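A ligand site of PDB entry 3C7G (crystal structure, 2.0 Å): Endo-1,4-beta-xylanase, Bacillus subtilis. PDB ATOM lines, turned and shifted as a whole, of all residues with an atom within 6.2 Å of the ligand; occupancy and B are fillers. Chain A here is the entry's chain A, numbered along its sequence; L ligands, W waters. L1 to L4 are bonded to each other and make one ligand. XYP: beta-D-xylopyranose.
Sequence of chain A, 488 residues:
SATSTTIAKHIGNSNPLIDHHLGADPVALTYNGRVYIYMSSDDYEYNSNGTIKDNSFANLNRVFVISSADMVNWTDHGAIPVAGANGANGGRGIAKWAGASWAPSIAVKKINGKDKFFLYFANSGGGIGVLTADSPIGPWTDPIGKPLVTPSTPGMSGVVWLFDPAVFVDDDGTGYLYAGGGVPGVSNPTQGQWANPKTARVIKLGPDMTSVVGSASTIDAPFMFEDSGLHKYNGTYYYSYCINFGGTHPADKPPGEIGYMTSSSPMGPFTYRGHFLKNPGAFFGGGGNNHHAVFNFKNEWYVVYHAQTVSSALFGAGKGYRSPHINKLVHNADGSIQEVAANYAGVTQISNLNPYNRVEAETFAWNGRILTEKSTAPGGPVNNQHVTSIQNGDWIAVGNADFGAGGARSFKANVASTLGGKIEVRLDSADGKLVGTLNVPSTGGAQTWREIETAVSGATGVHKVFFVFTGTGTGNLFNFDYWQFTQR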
ATOM      1  N   PHE A  57      22.285 -18.703 -25.066  1.00  0.00           N
ATOM      2  CA  PHE A  57      22.786 -17.744 -26.063  1.00  0.00           C
ATOM      3  C   PHE A  57      23.561 -18.397 -27.212  1.00  0.00           C
ATOM      4  O   PHE A  57      24.254 -17.709 -27.968  1.00  0.00           O
ATOM      5  CB  PHE A  57      23.648 -16.620 -25.451  1.00  0.00           C
ATOM      6  CG  PHE A  57      23.050 -15.965 -24.247  1.00  0.00           C
ATOM      7  CD1 PHE A  57      21.670 -15.779 -24.125  1.00  0.00           C
ATOM      8  CD2 PHE A  57      23.892 -15.528 -23.219  1.00  0.00           C
ATOM      9  CE1 PHE A  57      21.119 -15.170 -22.980  1.00  0.00           C
ATOM     10  CE2 PHE A  57      23.362 -14.927 -22.063  1.00  0.00           C
ATOM     11  CZ  PHE A  57      21.983 -14.739 -21.951  1.00  0.00           C
ATOM     12  N   TRP A 102      26.069 -10.310 -30.152  1.00  0.00           N
ATOM     13  CA  TRP A 102      25.064 -10.037 -29.113  1.00  0.00           C
ATOM     14  C   TRP A 102      24.757  -8.554 -29.088  1.00  0.00           C
ATOM     15  O   TRP A 102      25.663  -7.742 -29.244  1.00  0.00           O
ATOM     16  CB  TRP A 102      25.587 -10.370 -27.702  1.00  0.00           C
ATOM     17  CG  TRP A 102      25.865 -11.808 -27.402  1.00  0.00           C
ATOM     18  CD1 TRP A 102      25.797 -12.875 -28.270  1.00  0.00           C
ATOM     19  CD2 TRP A 102      26.314 -12.347 -26.145  1.00  0.00           C
ATOM     20  NE1 TRP A 102      26.150 -14.039 -27.608  1.00  0.00           N
ATOM     21  CE2 TRP A 102      26.457 -13.742 -26.303  1.00  0.00           C
ATOM     22  CE3 TRP A 102      26.571 -11.778 -24.884  1.00  0.00           C
ATOM     23  CZ2 TRP A 102      26.905 -14.581 -25.270  1.00  0.00           C
ATOM     24  CZ3 TRP A 102      26.995 -12.614 -23.842  1.00  0.00           C
ATOM     25  CH2 TRP A 102      27.139 -14.018 -24.045  1.00  0.00           C
ATOM     26  N   SER A 124      30.092 -12.002 -27.851  1.00  0.00           N
ATOM     27  CA  SER A 124      29.857 -12.363 -26.433  1.00  0.00           C
ATOM     28  C   SER A 124      30.389 -11.289 -25.459  1.00  0.00           C
ATOM     29  O   SER A 124      30.157 -10.094 -25.645  1.00  0.00           O
ATOM     30  CB  SER A 124      30.414 -13.756 -26.094  1.00  0.00           C
ATOM     31  OG  SER A 124      30.042 -14.700 -27.082  1.00  0.00           O
ATOM     32  N   GLY A 125      31.141 -11.719 -24.445  1.00  0.00           N
ATOM     33  CA  GLY A 125      31.629 -10.830 -23.405  1.00  0.00           C
ATOM     34  C   GLY A 125      33.042 -10.340 -23.640  1.00  0.00           C
ATOM     35  O   GLY A 125      33.665  -9.725 -22.737  1.00  0.00           O
ATOM     36  N   GLY A 126      33.557 -10.578 -24.860  1.00  0.00           N
ATOM     37  CA  GLY A 126      34.956 -10.313 -25.163  1.00  0.00           C
ATOM     38  C   GLY A 126      35.369  -9.132 -26.033  1.00  0.00           C
ATOM     39  O   GLY A 126      36.529  -8.740 -26.026  1.00  0.00           O
ATOM     40  N   VAL A 160      34.474  -6.245 -16.768  1.00  0.00           N
ATOM     41  CA  VAL A 160      34.258  -7.679 -16.564  1.00  0.00           C
ATOM     42  C   VAL A 160      33.632  -8.313 -17.821  1.00  0.00           C
ATOM     43  O   VAL A 160      34.143  -9.297 -18.377  1.00  0.00           O
ATOM     44  CB  VAL A 160      33.431  -7.974 -15.280  1.00  0.00           C
ATOM     45  CG1 VAL A 160      32.913  -9.447 -15.245  1.00  0.00           C
ATOM     46  CG2 VAL A 160      34.267  -7.669 -14.018  1.00  0.00           C
ATOM     47  N   TRP A 161      32.529  -7.717 -18.309  1.00  0.00           N
ATOM     48  CA  TRP A 161      31.896  -8.191 -19.530  1.00  0.00           C
ATOM     49  C   TRP A 161      31.945  -7.092 -20.568  1.00  0.00           C
ATOM     50  O   TRP A 161      31.245  -6.073 -20.436  1.00  0.00           O
ATOM     51  CB  TRP A 161      30.440  -8.595 -19.275  1.00  0.00           C
ATOM     52  CG  TRP A 161      30.252  -9.795 -18.370  1.00  0.00           C
ATOM     53  CD1 TRP A 161      31.127 -10.837 -18.180  1.00  0.00           C
ATOM     54  CD2 TRP A 161      29.082 -10.099 -17.617  1.00  0.00           C
ATOM     55  NE1 TRP A 161      30.580 -11.757 -17.314  1.00  0.00           N
ATOM     56  CE2 TRP A 161      29.318 -11.337 -16.961  1.00  0.00           C
ATOM     57  CE3 TRP A 161      27.851  -9.437 -17.409  1.00  0.00           C
ATOM     58  CZ2 TRP A 161      28.370 -11.920 -16.113  1.00  0.00           C
ATOM     59  CZ3 TRP A 161      26.919 -10.029 -16.573  1.00  0.00           C
ATOM     60  CH2 TRP A 161      27.187 -11.261 -15.931  1.00  0.00           C
ATOM     61  N   PHE A 163      30.755  -5.932 -23.360  1.00  0.00           N
ATOM     62  CA  PHE A 163      29.635  -6.202 -24.261  1.00  0.00           C
ATOM     63  C   PHE A 163      28.562  -5.102 -24.198  1.00  0.00           C
ATOM     64  O   PHE A 163      28.838  -3.998 -23.733  1.00  0.00           O
ATOM     65  CB  PHE A 163      29.112  -7.641 -24.058  1.00  0.00           C
ATOM     66  CG  PHE A 163      28.332  -7.865 -22.778  1.00  0.00           C
ATOM     67  CD1 PHE A 163      27.752  -9.111 -22.548  1.00  0.00           C
ATOM     68  CD2 PHE A 163      28.190  -6.873 -21.814  1.00  0.00           C
ATOM     69  CE1 PHE A 163      27.013  -9.348 -21.393  1.00  0.00           C
ATOM     70  CE2 PHE A 163      27.449  -7.080 -20.660  1.00  0.00           C
ATOM     71  CZ  PHE A 163      26.845  -8.319 -20.463  1.00  0.00           C
ATOM     72  N   ASP A 164      27.371  -5.416 -24.701  1.00  0.00           N
ATOM     73  CA  ASP A 164      26.241  -4.501 -24.678  1.00  0.00           C
ATOM     74  C   ASP A 164      26.632  -3.107 -25.132  1.00  0.00           C
ATOM     75  O   ASP A 164      26.562  -2.161 -24.350  1.00  0.00           O
ATOM     76  CB  ASP A 164      25.570  -4.503 -23.288  1.00  0.00           C
ATOM     77  CG  ASP A 164      24.827  -5.808 -23.002  1.00  0.00           C
ATOM     78  OD1 ASP A 164      24.978  -6.782 -23.792  1.00  0.00           O
ATOM     79  OD2 ASP A 164      24.075  -5.866 -22.016  1.00  0.00           O
ATOM     80  N   PHE A 225      25.201  -3.472 -14.096  1.00  0.00           N
ATOM     81  CA  PHE A 225      25.253  -4.857 -14.557  1.00  0.00           C
ATOM     82  C   PHE A 225      25.596  -4.995 -16.054  1.00  0.00           C
ATOM     83  O   PHE A 225      26.538  -5.680 -16.433  1.00  0.00           O
ATOM     84  CB  PHE A 225      23.960  -5.590 -14.230  1.00  0.00           C
ATOM     85  CG  PHE A 225      24.069  -7.089 -14.265  1.00  0.00           C
ATOM     86  CD1 PHE A 225      25.185  -7.740 -13.708  1.00  0.00           C
ATOM     87  CD2 PHE A 225      23.060  -7.865 -14.827  1.00  0.00           C
ATOM     88  CE1 PHE A 225      25.280  -9.148 -13.729  1.00  0.00           C
ATOM     89  CE2 PHE A 225      23.150  -9.277 -14.860  1.00  0.00           C
ATOM     90  CZ  PHE A 225      24.252  -9.913 -14.311  1.00  0.00           C
ATOM     91  N   GLU A 226      24.783  -4.381 -16.907  1.00  0.00           N
ATOM     92  CA  GLU A 226      24.928  -4.558 -18.358  1.00  0.00           C
ATOM     93  C   GLU A 226      23.985  -3.560 -19.043  1.00  0.00           C
ATOM     94  O   GLU A 226      23.423  -2.696 -18.392  1.00  0.00           O
ATOM     95  CB  GLU A 226      24.549  -5.995 -18.745  1.00  0.00           C
ATOM     96  CG  GLU A 226      23.187  -6.437 -18.195  1.00  0.00           C
ATOM     97  CD  GLU A 226      22.827  -7.862 -18.618  1.00  0.00           C
ATOM     98  OE1 GLU A 226      23.307  -8.269 -19.692  1.00  0.00           O
ATOM     99  OE2 GLU A 226      22.060  -8.539 -17.899  1.00  0.00           O
ATOM    100  N   PHE A 245      21.733  -7.899  -9.825  1.00  0.00           N
ATOM    101  CA  PHE A 245      20.764  -8.623  -9.031  1.00  0.00           C
ATOM    102  C   PHE A 245      21.295  -9.021  -7.648  1.00  0.00           C
ATOM    103  O   PHE A 245      20.536  -9.562  -6.837  1.00  0.00           O
ATOM    104  CB  PHE A 245      20.302  -9.877  -9.786  1.00  0.00           C
ATOM    105  CG  PHE A 245      19.607  -9.591 -11.087  1.00  0.00           C
ATOM    106  CD1 PHE A 245      18.205  -9.578 -11.144  1.00  0.00           C
ATOM    107  CD2 PHE A 245      20.348  -9.335 -12.258  1.00  0.00           C
ATOM    108  CE1 PHE A 245      17.550  -9.334 -12.358  1.00  0.00           C
ATOM    109  CE2 PHE A 245      19.698  -9.054 -13.470  1.00  0.00           C
ATOM    110  CZ  PHE A 245      18.303  -9.064 -13.523  1.00  0.00           C
ATOM    111  N   GLY A 246      22.571  -8.790  -7.400  1.00  0.00           N
ATOM    112  CA  GLY A 246      23.217  -9.353  -6.207  1.00  0.00           C
ATOM    113  C   GLY A 246      23.473  -8.322  -5.146  1.00  0.00           C
ATOM    114  O   GLY A 246      23.402  -7.112  -5.411  1.00  0.00           O
ATOM    115  N   ASN A 279      12.132  -4.883 -13.911  1.00  0.00           N
ATOM    116  CA  ASN A 279      12.419  -6.136 -14.555  1.00  0.00           C
ATOM    117  C   ASN A 279      11.190  -6.632 -15.316  1.00  0.00           C
ATOM    118  O   ASN A 279      10.071  -6.498 -14.817  1.00  0.00           O
ATOM    119  CB  ASN A 279      12.848  -7.182 -13.522  1.00  0.00           C
ATOM    120  CG  ASN A 279      13.554  -8.342 -14.177  1.00  0.00           C
ATOM    121  OD1 ASN A 279      12.925  -9.336 -14.520  1.00  0.00           O
ATOM    122  ND2 ASN A 279      14.866  -8.202 -14.433  1.00  0.00           N
ATOM    123  N   GLY A 286       8.382 -14.127 -14.218  1.00  0.00           N
ATOM    124  CA  GLY A 286       9.156 -13.393 -13.217  1.00  0.00           C
ATOM    125  C   GLY A 286      10.391 -14.287 -13.282  1.00  0.00           C
ATOM    126  O   GLY A 286      10.444 -15.289 -12.529  1.00  0.00           O
ATOM    127  N   GLY A 287      11.406 -14.029 -14.132  1.00  0.00           N
ATOM    128  CA  GLY A 287      11.836 -12.768 -14.756  1.00  0.00           C
ATOM    129  C   GLY A 287      13.178 -13.127 -15.428  1.00  0.00           C
ATOM    130  O   GLY A 287      13.419 -14.308 -15.741  1.00  0.00           O
ATOM    131  N   GLY A 288      14.075 -12.164 -15.625  1.00  0.00           N
ATOM    132  CA  GLY A 288      15.362 -12.465 -16.287  1.00  0.00           C
ATOM    133  C   GLY A 288      16.188 -11.221 -16.538  1.00  0.00           C
ATOM    134  O   GLY A 288      16.046 -10.211 -15.820  1.00  0.00           O
ATOM    135  N   ASN A 289      17.067 -11.262 -17.525  1.00  0.00           N
ATOM    136  CA  ASN A 289      17.823 -10.073 -17.864  1.00  0.00           C
ATOM    137  C   ASN A 289      16.935  -9.042 -18.542  1.00  0.00           C
ATOM    138  O   ASN A 289      15.881  -9.326 -19.112  1.00  0.00           O
ATOM    139  CB  ASN A 289      19.109 -10.356 -18.668  1.00  0.00           C
ATOM    140  CG  ASN A 289      18.856 -11.153 -19.932  1.00  0.00           C
ATOM    141  OD1 ASN A 289      18.038 -10.781 -20.763  1.00  0.00           O
ATOM    142  ND2 ASN A 289      19.578 -12.253 -20.084  1.00  0.00           N
ATOM    143  N   ASN A 290      17.408  -7.822 -18.479  1.00  0.00           N
ATOM    144  CA  ASN A 290      16.585  -6.726 -18.846  1.00  0.00           C
ATOM    145  C   ASN A 290      17.360  -5.719 -19.635  1.00  0.00           C
ATOM    146  O   ASN A 290      18.524  -5.474 -19.313  1.00  0.00           O
ATOM    147  CB  ASN A 290      16.202  -6.038 -17.509  1.00  0.00           C
ATOM    148  CG  ASN A 290      15.151  -4.929 -17.650  1.00  0.00           C
ATOM    149  OD1 ASN A 290      14.612  -4.673 -18.740  1.00  0.00           O
ATOM    150  ND2 ASN A 290      14.864  -4.270 -16.519  1.00  0.00           N
ATOM    151  N   GLN A 308      10.102 -12.169 -21.851  1.00  0.00           N
ATOM    152  CA  GLN A 308       9.927 -13.547 -22.277  1.00  0.00           C
ATOM    153  C   GLN A 308       8.468 -13.891 -22.604  1.00  0.00           C
ATOM    154  O   GLN A 308       7.955 -14.937 -22.223  1.00  0.00           O
ATOM    155  CB  GLN A 308      10.509 -14.494 -21.206  1.00  0.00           C
ATOM    156  CG  GLN A 308      11.988 -14.201 -20.901  1.00  0.00           C
ATOM    157  CD  GLN A 308      12.479 -15.038 -19.726  1.00  0.00           C
ATOM    158  OE1 GLN A 308      12.384 -16.253 -19.737  1.00  0.00           O
ATOM    159  NE2 GLN A 308      12.939 -14.383 -18.706  1.00  0.00           N
ATOM    160  N   ARG A 322      13.607 -14.335 -25.546  1.00  0.00           N
ATOM    161  CA  ARG A 322      13.113 -12.984 -25.374  1.00  0.00           C
ATOM    162  C   ARG A 322      12.533 -12.380 -26.640  1.00  0.00           C
ATOM    163  O   ARG A 322      12.890 -12.738 -27.769  1.00  0.00           O
ATOM    164  CB  ARG A 322      14.220 -12.096 -24.788  1.00  0.00           C
ATOM    165  CG  ARG A 322      14.637 -12.526 -23.356  1.00  0.00           C
ATOM    166  CD  ARG A 322      16.110 -12.324 -23.121  1.00  0.00           C
ATOM    167  NE  ARG A 322      16.967 -12.943 -24.154  1.00  0.00           N
ATOM    168  CZ  ARG A 322      18.279 -12.699 -24.254  1.00  0.00           C
ATOM    169  NH1 ARG A 322      19.029 -13.269 -25.213  1.00  0.00           N
ATOM    170  NH2 ARG A 322      18.827 -11.871 -23.403  1.00  0.00           N
HETATM  171  O1  XYP L   1      13.310 -13.111 -10.342  1.00  0.00           O
HETATM  172  C1  XYP L   1      14.619 -13.636 -10.542  1.00  0.00           C
HETATM  173  C2  XYP L   1      14.691 -14.004 -12.016  1.00  0.00           C
HETATM  174  C3  XYP L   1      16.101 -14.388 -12.371  1.00  0.00           C
HETATM  175  C4  XYP L   1      17.048 -13.272 -11.991  1.00  0.00           C
HETATM  176  C5  XYP L   1      16.925 -12.869 -10.524  1.00  0.00           C
HETATM  177  O2  XYP L   1      13.865 -15.132 -12.288  1.00  0.00           O
HETATM  178  O3  XYP L   1      16.188 -14.671 -13.776  1.00  0.00           O
HETATM  179  O4  XYP L   1      18.346 -13.789 -12.221  1.00  0.00           O
HETATM  180  O5  XYP L   1      15.551 -12.592 -10.227  1.00  0.00           O
HETATM  181  C1  XYP L   2      19.296 -12.975 -13.159  1.00  0.00           C
HETATM  182  C2  XYP L   2      20.700 -13.470 -12.853  1.00  0.00           C
HETATM  183  C3  XYP L   2      21.642 -12.757 -13.800  1.00  0.00           C
HETATM  184  C4  XYP L   2      21.146 -12.853 -15.250  1.00  0.00           C
HETATM  185  C5  XYP L   2      19.743 -12.313 -15.426  1.00  0.00           C
HETATM  186  O2  XYP L   2      21.051 -13.110 -11.525  1.00  0.00           O
HETATM  187  O3  XYP L   2      22.939 -13.308 -13.673  1.00  0.00           O
HETATM  188  O4  XYP L   2      22.002 -12.030 -16.040  1.00  0.00           O
HETATM  189  O5  XYP L   2      18.929 -13.082 -14.552  1.00  0.00           O
HETATM  190  C1  XYP L   3      22.775 -12.682 -17.220  1.00  0.00           C
HETATM  191  C2  XYP L   3      23.353 -11.625 -18.146  1.00  0.00           C
HETATM  192  C3  XYP L   3      24.254 -12.407 -19.085  1.00  0.00           C
HETATM  193  C4  XYP L   3      25.242 -13.245 -18.273  1.00  0.00           C
HETATM  194  C5  XYP L   3      24.638 -14.096 -17.143  1.00  0.00           C
HETATM  195  O2  XYP L   3      22.291 -10.953 -18.838  1.00  0.00           O
HETATM  196  O3  XYP L   3      25.010 -11.496 -19.904  1.00  0.00           O
HETATM  197  O4  XYP L   3      25.898 -14.098 -19.223  1.00  0.00           O
HETATM  198  O5  XYP L   3      23.794 -13.239 -16.375  1.00  0.00           O
HETATM  199  C1  XYP L   4      27.489 -13.702 -19.273  1.00  0.00           C
HETATM  200  C2  XYP L   4      27.974 -15.005 -19.884  1.00  0.00           C
HETATM  201  C3  XYP L   4      29.445 -14.764 -20.184  1.00  0.00           C
HETATM  202  C4  XYP L   4      29.561 -13.583 -21.126  1.00  0.00           C
HETATM  203  C5  XYP L   4      28.766 -12.362 -20.664  1.00  0.00           C
HETATM  204  O2  XYP L   4      27.762 -16.039 -18.923  1.00  0.00           O
HETATM  205  O3  XYP L   4      29.879 -15.935 -20.836  1.00  0.00           O
HETATM  206  O4  XYP L   4      30.927 -13.192 -21.154  1.00  0.00           O
HETATM  207  O5  XYP L   4      27.426 -12.749 -20.326  1.00  0.00           O
HETATM  208  O   HOH W   1      23.341 -12.129 -10.701  1.00  0.00           O
HETATM  209  O   HOH W   2      24.963 -17.509 -19.538  1.00  0.00           O
HETATM  210  O   HOH W   3      19.846 -14.519 -17.991  1.00  0.00           O
HETATM  211  O   HOH W   4      26.184 -14.492 -14.017  1.00  0.00           O
HETATM  212  O   HOH W   5      28.417 -17.069 -22.950  1.00  0.00           O
HETATM  213  O   HOH W   6      32.933 -13.580 -19.246  1.00  0.00           O
HETATM  214  O   HOH W   7      32.220 -14.305 -23.125  1.00  0.00           O
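Residues that only touch the ligand: Phe 225 (3.2 Å), Phe 163 (3.3 Å), Gly 125 (3.3 Å), Gly 288 (3.4 Å), Trp 102 (3.5 Å), Phe 245 (3.6 Å), Trp 161 (3.6 Å) and Phe 57 (3.9 Å).
Hydrophobic or aromatic side chains within 4 Å of the ligand: Phe 57, Trp 102, Trp 161, Phe 163, Phe 225 and Phe 245.
Of the 21 residues printed, 12 come within 4 Å of the ligand.
The nearest printed residue that does not touch the ligand is Ser 124 (4.7 Å).
OD1 of Asn 289 is in hydrogen-bond range of NH2 of Arg 322, at 3.0 Å.
NE2 of Gln 308 is in hydrogen-bond range of O of Gly 287, 3.0 Å away.
O of Gly 288 lies within hydrogen-bond range of ND2 of Asn 279 (2.7 Å).
Water W7 bridges O4 of XYP L4 (2.6 Å) and N of Gly 125 (3.1 Å).
O2 of XYP L3 sits at hydrogen-bond distance from OE2 of Glu 226, at 2.6 Å.
An oxygen (O2) of XYP L3 sits close to the side-chain amide nitrogen of Asn 289, 3.3 Å away.
An oxygen (O2) of XYP L1 is in hydrogen-bond range of the backbone NH of Gly 287, at 3.3 Å.
The backbone carbonyl oxygen (O) of Gly 287 lies within hydrogen-bond range of an oxygen (O3) of XYP L1 (3.4 Å).
An oxygen (O2) of XYP L1 lies within hydrogen-bond range of the backbone carbonyl oxygen of Gly 286 (3.4 Å).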
